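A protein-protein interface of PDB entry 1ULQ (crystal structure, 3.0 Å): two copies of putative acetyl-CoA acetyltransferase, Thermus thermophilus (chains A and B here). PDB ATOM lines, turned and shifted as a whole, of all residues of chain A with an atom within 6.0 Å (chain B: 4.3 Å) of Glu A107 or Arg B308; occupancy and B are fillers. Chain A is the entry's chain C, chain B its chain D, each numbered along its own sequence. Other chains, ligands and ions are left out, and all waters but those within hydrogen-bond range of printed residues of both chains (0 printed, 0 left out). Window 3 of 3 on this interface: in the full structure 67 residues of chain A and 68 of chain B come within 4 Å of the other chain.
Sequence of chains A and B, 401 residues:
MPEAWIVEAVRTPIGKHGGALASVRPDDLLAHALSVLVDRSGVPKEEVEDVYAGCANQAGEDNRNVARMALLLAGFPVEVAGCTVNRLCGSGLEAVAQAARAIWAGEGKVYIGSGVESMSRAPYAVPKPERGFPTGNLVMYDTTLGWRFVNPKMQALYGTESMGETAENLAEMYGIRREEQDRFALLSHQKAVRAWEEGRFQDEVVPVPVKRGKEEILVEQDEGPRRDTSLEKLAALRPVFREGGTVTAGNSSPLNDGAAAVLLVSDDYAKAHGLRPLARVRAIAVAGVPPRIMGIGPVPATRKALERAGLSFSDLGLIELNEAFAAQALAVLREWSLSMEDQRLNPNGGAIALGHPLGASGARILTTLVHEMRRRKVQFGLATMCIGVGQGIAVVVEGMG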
ATOM      1  N   GLU A  49      19.076  -7.015 -24.792  1.00  0.00           N
ATOM      2  CA  GLU A  49      18.528  -6.442 -23.572  1.00  0.00           C
ATOM      3  C   GLU A  49      17.910  -7.475 -22.633  1.00  0.00           C
ATOM      4  O   GLU A  49      18.200  -7.500 -21.436  1.00  0.00           O
ATOM      5  CB  GLU A  49      17.467  -5.421 -23.961  1.00  0.00           C
ATOM      6  CG  GLU A  49      16.711  -4.782 -22.828  1.00  0.00           C
ATOM      7  CD  GLU A  49      17.577  -3.880 -21.997  1.00  0.00           C
ATOM      8  OE1 GLU A  49      18.650  -3.460 -22.487  1.00  0.00           O
ATOM      9  OE2 GLU A  49      17.175  -3.582 -20.856  1.00  0.00           O
ATOM     10  N   TYR A  52      13.102 -13.445 -23.858  1.00  0.00           N
ATOM     11  CA  TYR A  52      11.838 -14.062 -23.488  1.00  0.00           C
ATOM     12  C   TYR A  52      11.800 -15.436 -24.127  1.00  0.00           C
ATOM     13  O   TYR A  52      12.253 -15.612 -25.257  1.00  0.00           O
ATOM     14  CB  TYR A  52      10.636 -13.250 -23.990  1.00  0.00           C
ATOM     15  CG  TYR A  52      10.358 -11.983 -23.215  1.00  0.00           C
ATOM     16  CD1 TYR A  52      10.653 -10.733 -23.759  1.00  0.00           C
ATOM     17  CD2 TYR A  52       9.773 -12.028 -21.951  1.00  0.00           C
ATOM     18  CE1 TYR A  52      10.367  -9.555 -23.068  1.00  0.00           C
ATOM     19  CE2 TYR A  52       9.483 -10.854 -21.252  1.00  0.00           C
ATOM     20  CZ  TYR A  52       9.781  -9.623 -21.820  1.00  0.00           C
ATOM     21  OH  TYR A  52       9.481  -8.454 -21.154  1.00  0.00           O
ATOM     22  N   ALA A 102       7.963  -4.495 -25.587  1.00  0.00           N
ATOM     23  CA  ALA A 102       9.027  -3.815 -24.849  1.00  0.00           C
ATOM     24  C   ALA A 102       9.718  -2.794 -25.767  1.00  0.00           C
ATOM     25  O   ALA A 102      10.044  -1.678 -25.356  1.00  0.00           O
ATOM     26  CB  ALA A 102      10.043  -4.834 -24.337  1.00  0.00           C
ATOM     27  N   ILE A 103       9.942  -3.196 -27.014  1.00  0.00           N
ATOM     28  CA  ILE A 103      10.577  -2.340 -27.994  1.00  0.00           C
ATOM     29  C   ILE A 103       9.670  -1.144 -28.261  1.00  0.00           C
ATOM     30  O   ILE A 103      10.152  -0.026 -28.400  1.00  0.00           O
ATOM     31  CB  ILE A 103      10.851  -3.129 -29.286  1.00  0.00           C
ATOM     32  CG1 ILE A 103      11.879  -4.227 -28.993  1.00  0.00           C
ATOM     33  CG2 ILE A 103      11.347  -2.213 -30.374  1.00  0.00           C
ATOM     34  CD1 ILE A 103      12.207  -5.102 -30.180  1.00  0.00           C
ATOM     35  N   TRP A 104       8.361  -1.368 -28.307  1.00  0.00           N
ATOM     36  CA  TRP A 104       7.413  -0.277 -28.531  1.00  0.00           C
ATOM     37  C   TRP A 104       7.402   0.686 -27.339  1.00  0.00           C
ATOM     38  O   TRP A 104       7.179   1.886 -27.503  1.00  0.00           O
ATOM     39  CB  TRP A 104       5.982  -0.796 -28.731  1.00  0.00           C
ATOM     40  CG  TRP A 104       5.735  -1.606 -29.974  1.00  0.00           C
ATOM     41  CD1 TRP A 104       6.466  -1.596 -31.128  1.00  0.00           C
ATOM     42  CD2 TRP A 104       4.655  -2.524 -30.194  1.00  0.00           C
ATOM     43  NE1 TRP A 104       5.909  -2.452 -32.054  1.00  0.00           N
ATOM     44  CE2 TRP A 104       4.795  -3.033 -31.506  1.00  0.00           C
ATOM     45  CE3 TRP A 104       3.576  -2.966 -29.406  1.00  0.00           C
ATOM     46  CZ2 TRP A 104       3.899  -3.959 -32.050  1.00  0.00           C
ATOM     47  CZ3 TRP A 104       2.683  -3.891 -29.947  1.00  0.00           C
ATOM     48  CH2 TRP A 104       2.853  -4.376 -31.258  1.00  0.00           C
ATOM     49  N   ALA A 105       7.619   0.153 -26.140  1.00  0.00           N
ATOM     50  CA  ALA A 105       7.644   0.969 -24.928  1.00  0.00           C
ATOM     51  C   ALA A 105       8.934   1.775 -24.842  1.00  0.00           C
ATOM     52  O   ALA A 105       9.126   2.552 -23.903  1.00  0.00           O
ATOM     53  CB  ALA A 105       7.508   0.096 -23.701  1.00  0.00           C
ATOM     54  N   GLY A 106       9.815   1.572 -25.816  1.00  0.00           N
ATOM     55  CA  GLY A 106      11.069   2.296 -25.855  1.00  0.00           C
ATOM     56  C   GLY A 106      12.037   1.999 -24.730  1.00  0.00           C
ATOM     57  O   GLY A 106      12.678   2.906 -24.199  1.00  0.00           O
ATOM     58  N   GLU A 107      12.158   0.736 -24.353  1.00  0.00           N
ATOM     59  CA  GLU A 107      13.082   0.394 -23.291  1.00  0.00           C
ATOM     60  C   GLU A 107      14.392   0.017 -23.958  1.00  0.00           C
ATOM     61  O   GLU A 107      15.223   0.875 -24.213  1.00  0.00           O
ATOM     62  CB  GLU A 107      12.534  -0.764 -22.456  1.00  0.00           C
ATOM     63  CG  GLU A 107      11.081  -0.584 -22.033  1.00  0.00           C
ATOM     64  CD  GLU A 107      10.642  -1.602 -20.995  1.00  0.00           C
ATOM     65  OE1 GLU A 107      11.085  -2.775 -21.097  1.00  0.00           O
ATOM     66  OE2 GLU A 107       9.851  -1.229 -20.089  1.00  0.00           O
ATOM     67  N   GLY A 108      14.570  -1.260 -24.255  1.00  0.00           N
ATOM     68  CA  GLY A 108      15.799  -1.683 -24.892  1.00  0.00           C
ATOM     69  C   GLY A 108      15.660  -1.538 -26.388  1.00  0.00           C
ATOM     70  O   GLY A 108      14.617  -1.079 -26.862  1.00  0.00           O
ATOM     71  N   LYS A 109      16.694  -1.928 -27.130  1.00  0.00           N
ATOM     72  CA  LYS A 109      16.666  -1.831 -28.583  1.00  0.00           C
ATOM     73  C   LYS A 109      16.824  -3.185 -29.261  1.00  0.00           C
ATOM     74  O   LYS A 109      16.567  -3.332 -30.458  1.00  0.00           O
ATOM     75  CB  LYS A 109      17.764  -0.884 -29.060  1.00  0.00           C
ATOM     76  CG  LYS A 109      17.583   0.530 -28.543  1.00  0.00           C
ATOM     77  CD  LYS A 109      18.303   1.534 -29.401  1.00  0.00           C
ATOM     78  CE  LYS A 109      17.702   2.889 -29.180  1.00  0.00           C
ATOM     79  NZ  LYS A 109      16.239   2.876 -29.497  1.00  0.00           N
ATOM     80  N   TYR A 111      15.862  -7.315 -28.533  1.00  0.00           N
ATOM     81  CA  TYR A 111      15.212  -8.347 -27.722  1.00  0.00           C
ATOM     82  C   TYR A 111      15.105  -9.690 -28.448  1.00  0.00           C
ATOM     83  O   TYR A 111      15.087  -9.740 -29.677  1.00  0.00           O
ATOM     84  CB  TYR A 111      13.805  -7.905 -27.334  1.00  0.00           C
ATOM     85  CG  TYR A 111      13.725  -6.894 -26.212  1.00  0.00           C
ATOM     86  CD1 TYR A 111      14.076  -5.551 -26.404  1.00  0.00           C
ATOM     87  CD2 TYR A 111      13.259  -7.275 -24.956  1.00  0.00           C
ATOM     88  CE1 TYR A 111      13.952  -4.620 -25.358  1.00  0.00           C
ATOM     89  CE2 TYR A 111      13.133  -6.356 -23.914  1.00  0.00           C
ATOM     90  CZ  TYR A 111      13.474  -5.037 -24.116  1.00  0.00           C
ATOM     91  OH  TYR A 111      13.293  -4.158 -23.069  1.00  0.00           O
ATOM     92  N   ARG B 101       2.790  -2.713 -20.303  1.00  0.00           N
ATOM     93  CA  ARG B 101       3.248  -2.678 -21.692  1.00  0.00           C
ATOM     94  C   ARG B 101       2.173  -2.955 -22.725  1.00  0.00           C
ATOM     95  O   ARG B 101       2.266  -2.496 -23.871  1.00  0.00           O
ATOM     96  CB  ARG B 101       4.373  -3.670 -21.907  1.00  0.00           C
ATOM     97  CG  ARG B 101       5.578  -3.367 -21.084  1.00  0.00           C
ATOM     98  CD  ARG B 101       6.843  -3.332 -21.915  1.00  0.00           C
ATOM     99  NE  ARG B 101       7.966  -3.235 -21.005  1.00  0.00           N
ATOM    100  CZ  ARG B 101       8.402  -4.250 -20.274  1.00  0.00           C
ATOM    101  NH1 ARG B 101       7.817  -5.438 -20.371  1.00  0.00           N
ATOM    102  NH2 ARG B 101       9.385  -4.066 -19.405  1.00  0.00           N
ATOM    103  N   ALA B 283       7.907   4.001 -15.436  1.00  0.00           N
ATOM    104  CA  ALA B 283       8.918   3.312 -16.230  1.00  0.00           C
ATOM    105  C   ALA B 283       9.257   1.957 -15.659  1.00  0.00           C
ATOM    106  O   ALA B 283       9.084   1.727 -14.457  1.00  0.00           O
ATOM    107  CB  ALA B 283      10.184   4.158 -16.317  1.00  0.00           C
ATOM    108  N   ILE B 284       9.744   1.066 -16.520  1.00  0.00           N
ATOM    109  CA  ILE B 284      10.123  -0.274 -16.090  1.00  0.00           C
ATOM    110  C   ILE B 284      11.524  -0.589 -16.607  1.00  0.00           C
ATOM    111  O   ILE B 284      11.923  -0.106 -17.661  1.00  0.00           O
ATOM    112  CB  ILE B 284       9.161  -1.337 -16.644  1.00  0.00           C
ATOM    113  CG1 ILE B 284       7.716  -0.945 -16.364  1.00  0.00           C
ATOM    114  CG2 ILE B 284       9.425  -2.661 -15.976  1.00  0.00           C
ATOM    115  CD1 ILE B 284       6.731  -1.831 -17.062  1.00  0.00           C
ATOM    116  N   ALA B 285      12.271  -1.393 -15.864  1.00  0.00           N
ATOM    117  CA  ALA B 285      13.608  -1.756 -16.295  1.00  0.00           C
ATOM    118  C   ALA B 285      13.998  -3.095 -15.704  1.00  0.00           C
ATOM    119  O   ALA B 285      13.628  -3.420 -14.575  1.00  0.00           O
ATOM    120  CB  ALA B 285      14.605  -0.688 -15.884  1.00  0.00           C
ATOM    121  N   LYS B 304      18.461   2.097 -14.468  1.00  0.00           N
ATOM    122  CA  LYS B 304      17.845   2.105 -15.780  1.00  0.00           C
ATOM    123  C   LYS B 304      16.400   2.562 -15.745  1.00  0.00           C
ATOM    124  O   LYS B 304      15.921   3.196 -16.686  1.00  0.00           O
ATOM    125  CB  LYS B 304      17.920   0.720 -16.415  1.00  0.00           C
ATOM    126  CG  LYS B 304      19.307   0.354 -16.880  1.00  0.00           C
ATOM    127  CD  LYS B 304      19.270  -0.670 -18.021  1.00  0.00           C
ATOM    128  CE  LYS B 304      18.883  -2.072 -17.563  1.00  0.00           C
ATOM    129  NZ  LYS B 304      18.863  -3.039 -18.694  1.00  0.00           N
ATOM    130  N   ALA B 305      15.700   2.233 -14.664  1.00  0.00           N
ATOM    131  CA  ALA B 305      14.295   2.619 -14.530  1.00  0.00           C
ATOM    132  C   ALA B 305      14.177   4.123 -14.277  1.00  0.00           C
ATOM    133  O   ALA B 305      13.434   4.830 -14.967  1.00  0.00           O
ATOM    134  CB  ALA B 305      13.637   1.829 -13.394  1.00  0.00           C
ATOM    135  N   LEU B 306      14.917   4.601 -13.284  1.00  0.00           N
ATOM    136  CA  LEU B 306      14.911   6.008 -12.960  1.00  0.00           C
ATOM    137  C   LEU B 306      15.240   6.834 -14.201  1.00  0.00           C
ATOM    138  O   LEU B 306      14.584   7.838 -14.509  1.00  0.00           O
ATOM    139  CB  LEU B 306      15.919   6.273 -11.859  1.00  0.00           C
ATOM    140  CG  LEU B 306      15.288   6.112 -10.490  1.00  0.00           C
ATOM    141  CD1 LEU B 306      16.306   6.264  -9.366  1.00  0.00           C
ATOM    142  CD2 LEU B 306      14.203   7.161 -10.387  1.00  0.00           C
ATOM    143  N   GLU B 307      16.262   6.399 -14.921  1.00  0.00           N
ATOM    144  CA  GLU B 307      16.673   7.090 -16.126  1.00  0.00           C
ATOM    145  C   GLU B 307      15.554   7.087 -17.173  1.00  0.00           C
ATOM    146  O   GLU B 307      15.351   8.074 -17.873  1.00  0.00           O
ATOM    147  CB  GLU B 307      17.921   6.424 -16.677  1.00  0.00           C
ATOM    148  CG  GLU B 307      18.515   7.102 -17.872  1.00  0.00           C
ATOM    149  CD  GLU B 307      18.653   6.138 -19.019  1.00  0.00           C
ATOM    150  OE1 GLU B 307      17.671   5.998 -19.790  1.00  0.00           O
ATOM    151  OE2 GLU B 307      19.733   5.504 -19.133  1.00  0.00           O
ATOM    152  N   ARG B 308      14.820   5.983 -17.273  1.00  0.00           N
ATOM    153  CA  ARG B 308      13.733   5.890 -18.240  1.00  0.00           C
ATOM    154  C   ARG B 308      12.550   6.735 -17.812  1.00  0.00           C
ATOM    155  O   ARG B 308      11.703   7.095 -18.618  1.00  0.00           O
ATOM    156  CB  ARG B 308      13.291   4.435 -18.415  1.00  0.00           C
ATOM    157  CG  ARG B 308      14.283   3.585 -19.183  1.00  0.00           C
ATOM    158  CD  ARG B 308      13.842   2.145 -19.308  1.00  0.00           C
ATOM    159  NE  ARG B 308      14.734   1.395 -20.179  1.00  0.00           N
ATOM    160  CZ  ARG B 308      14.853   0.077 -20.164  1.00  0.00           C
ATOM    161  NH1 ARG B 308      14.135  -0.642 -19.320  1.00  0.00           N
ATOM    162  NH2 ARG B 308      15.699  -0.523 -20.983  1.00  0.00           N
ATOM    163  N   ALA B 309      12.484   7.045 -16.529  1.00  0.00           N
ATOM    164  CA  ALA B 309      11.387   7.864 -16.033  1.00  0.00           C
ATOM    165  C   ALA B 309      11.827   9.316 -15.958  1.00  0.00           C
ATOM    166  O   ALA B 309      11.025  10.193 -15.646  1.00  0.00           O
ATOM    167  CB  ALA B 309      10.953   7.391 -14.661  1.00  0.00           C
ATOM    168  N   GLY B 310      13.103   9.564 -16.240  1.00  0.00           N
ATOM    169  CA  GLY B 310      13.613  10.917 -16.183  1.00  0.00           C
ATOM    170  C   GLY B 310      13.568  11.468 -14.770  1.00  0.00           C
ATOM    171  O   GLY B 310      13.180  12.618 -14.538  1.00  0.00           O
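Arg B308 touches just these residues of chain A: Glu A49 (3.4 Å), Glu A107 (3.3 Å) and Gly A108 (3.5 Å).
Of the printed residues of chain B, Glu A49 touches Lys B304 and Arg B308.
Of the printed residues of chain A, Lys B304 touches Glu A49.
Of the printed residues of chain A, Ile B284 touches Glu A107.
Printed residues of chain B within 4 Å of Ala A102: Arg B101.
Of the printed residues of chain B, Gly A108 touches Arg B308.
The nearest printed residue of chain B that does not touch Tyr A52 is Ile B284 (7.8 Å).
Hydrophobic or aromatic side chains of chain B that line the printed part of chain A: Ile B284.
Hydrophobic or aromatic side chains of chain A within 4 Å of the printed part of chain B: Tyr A52 and Ala A105.
Among the printed residues, pairs that only touch across the chains: Glu A107 with Arg B308, Tyr A52 with Arg B101, Gly A108 with Arg B308, Ala A102 with Arg B101 and Ala A105 with Arg B101.
OE1 of Glu A107 lies within salt-bridge range of NH2 of Arg B101, 2.7 Å away.
OE2 of Glu A107 lies close to O of Ile B284 (3.4 Å).
The side-chain amino group (NZ) of Lys B304 is in salt-bridge range of the side-chain carboxylate (OE2) of Glu A49 (2.8 Å).
NH2 of Arg B308 is in salt-bridge range of OE2 of Glu A49 (3.4 Å).
No position is printed for both chains.
Of the 9 pairs that touch across the chains among the printed residues, none has its exchanged pair printed and touching as well.
The backbone carbonyl oxygen (O) of Ala A102 sits at hydrogen-bond distance from the backbone NH (N) of Glu A107, 3.4 Å away.
OE1 of Glu A107 sits at hydrogen-bond distance from OH of Tyr A111.
O of Ile B284 is in hydrogen-bond range of NH1 of Arg B308.
The side-chain hydroxyl (OH) of Tyr A111 lies within hydrogen-bond range of the backbone NH (N) of Gly A108.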
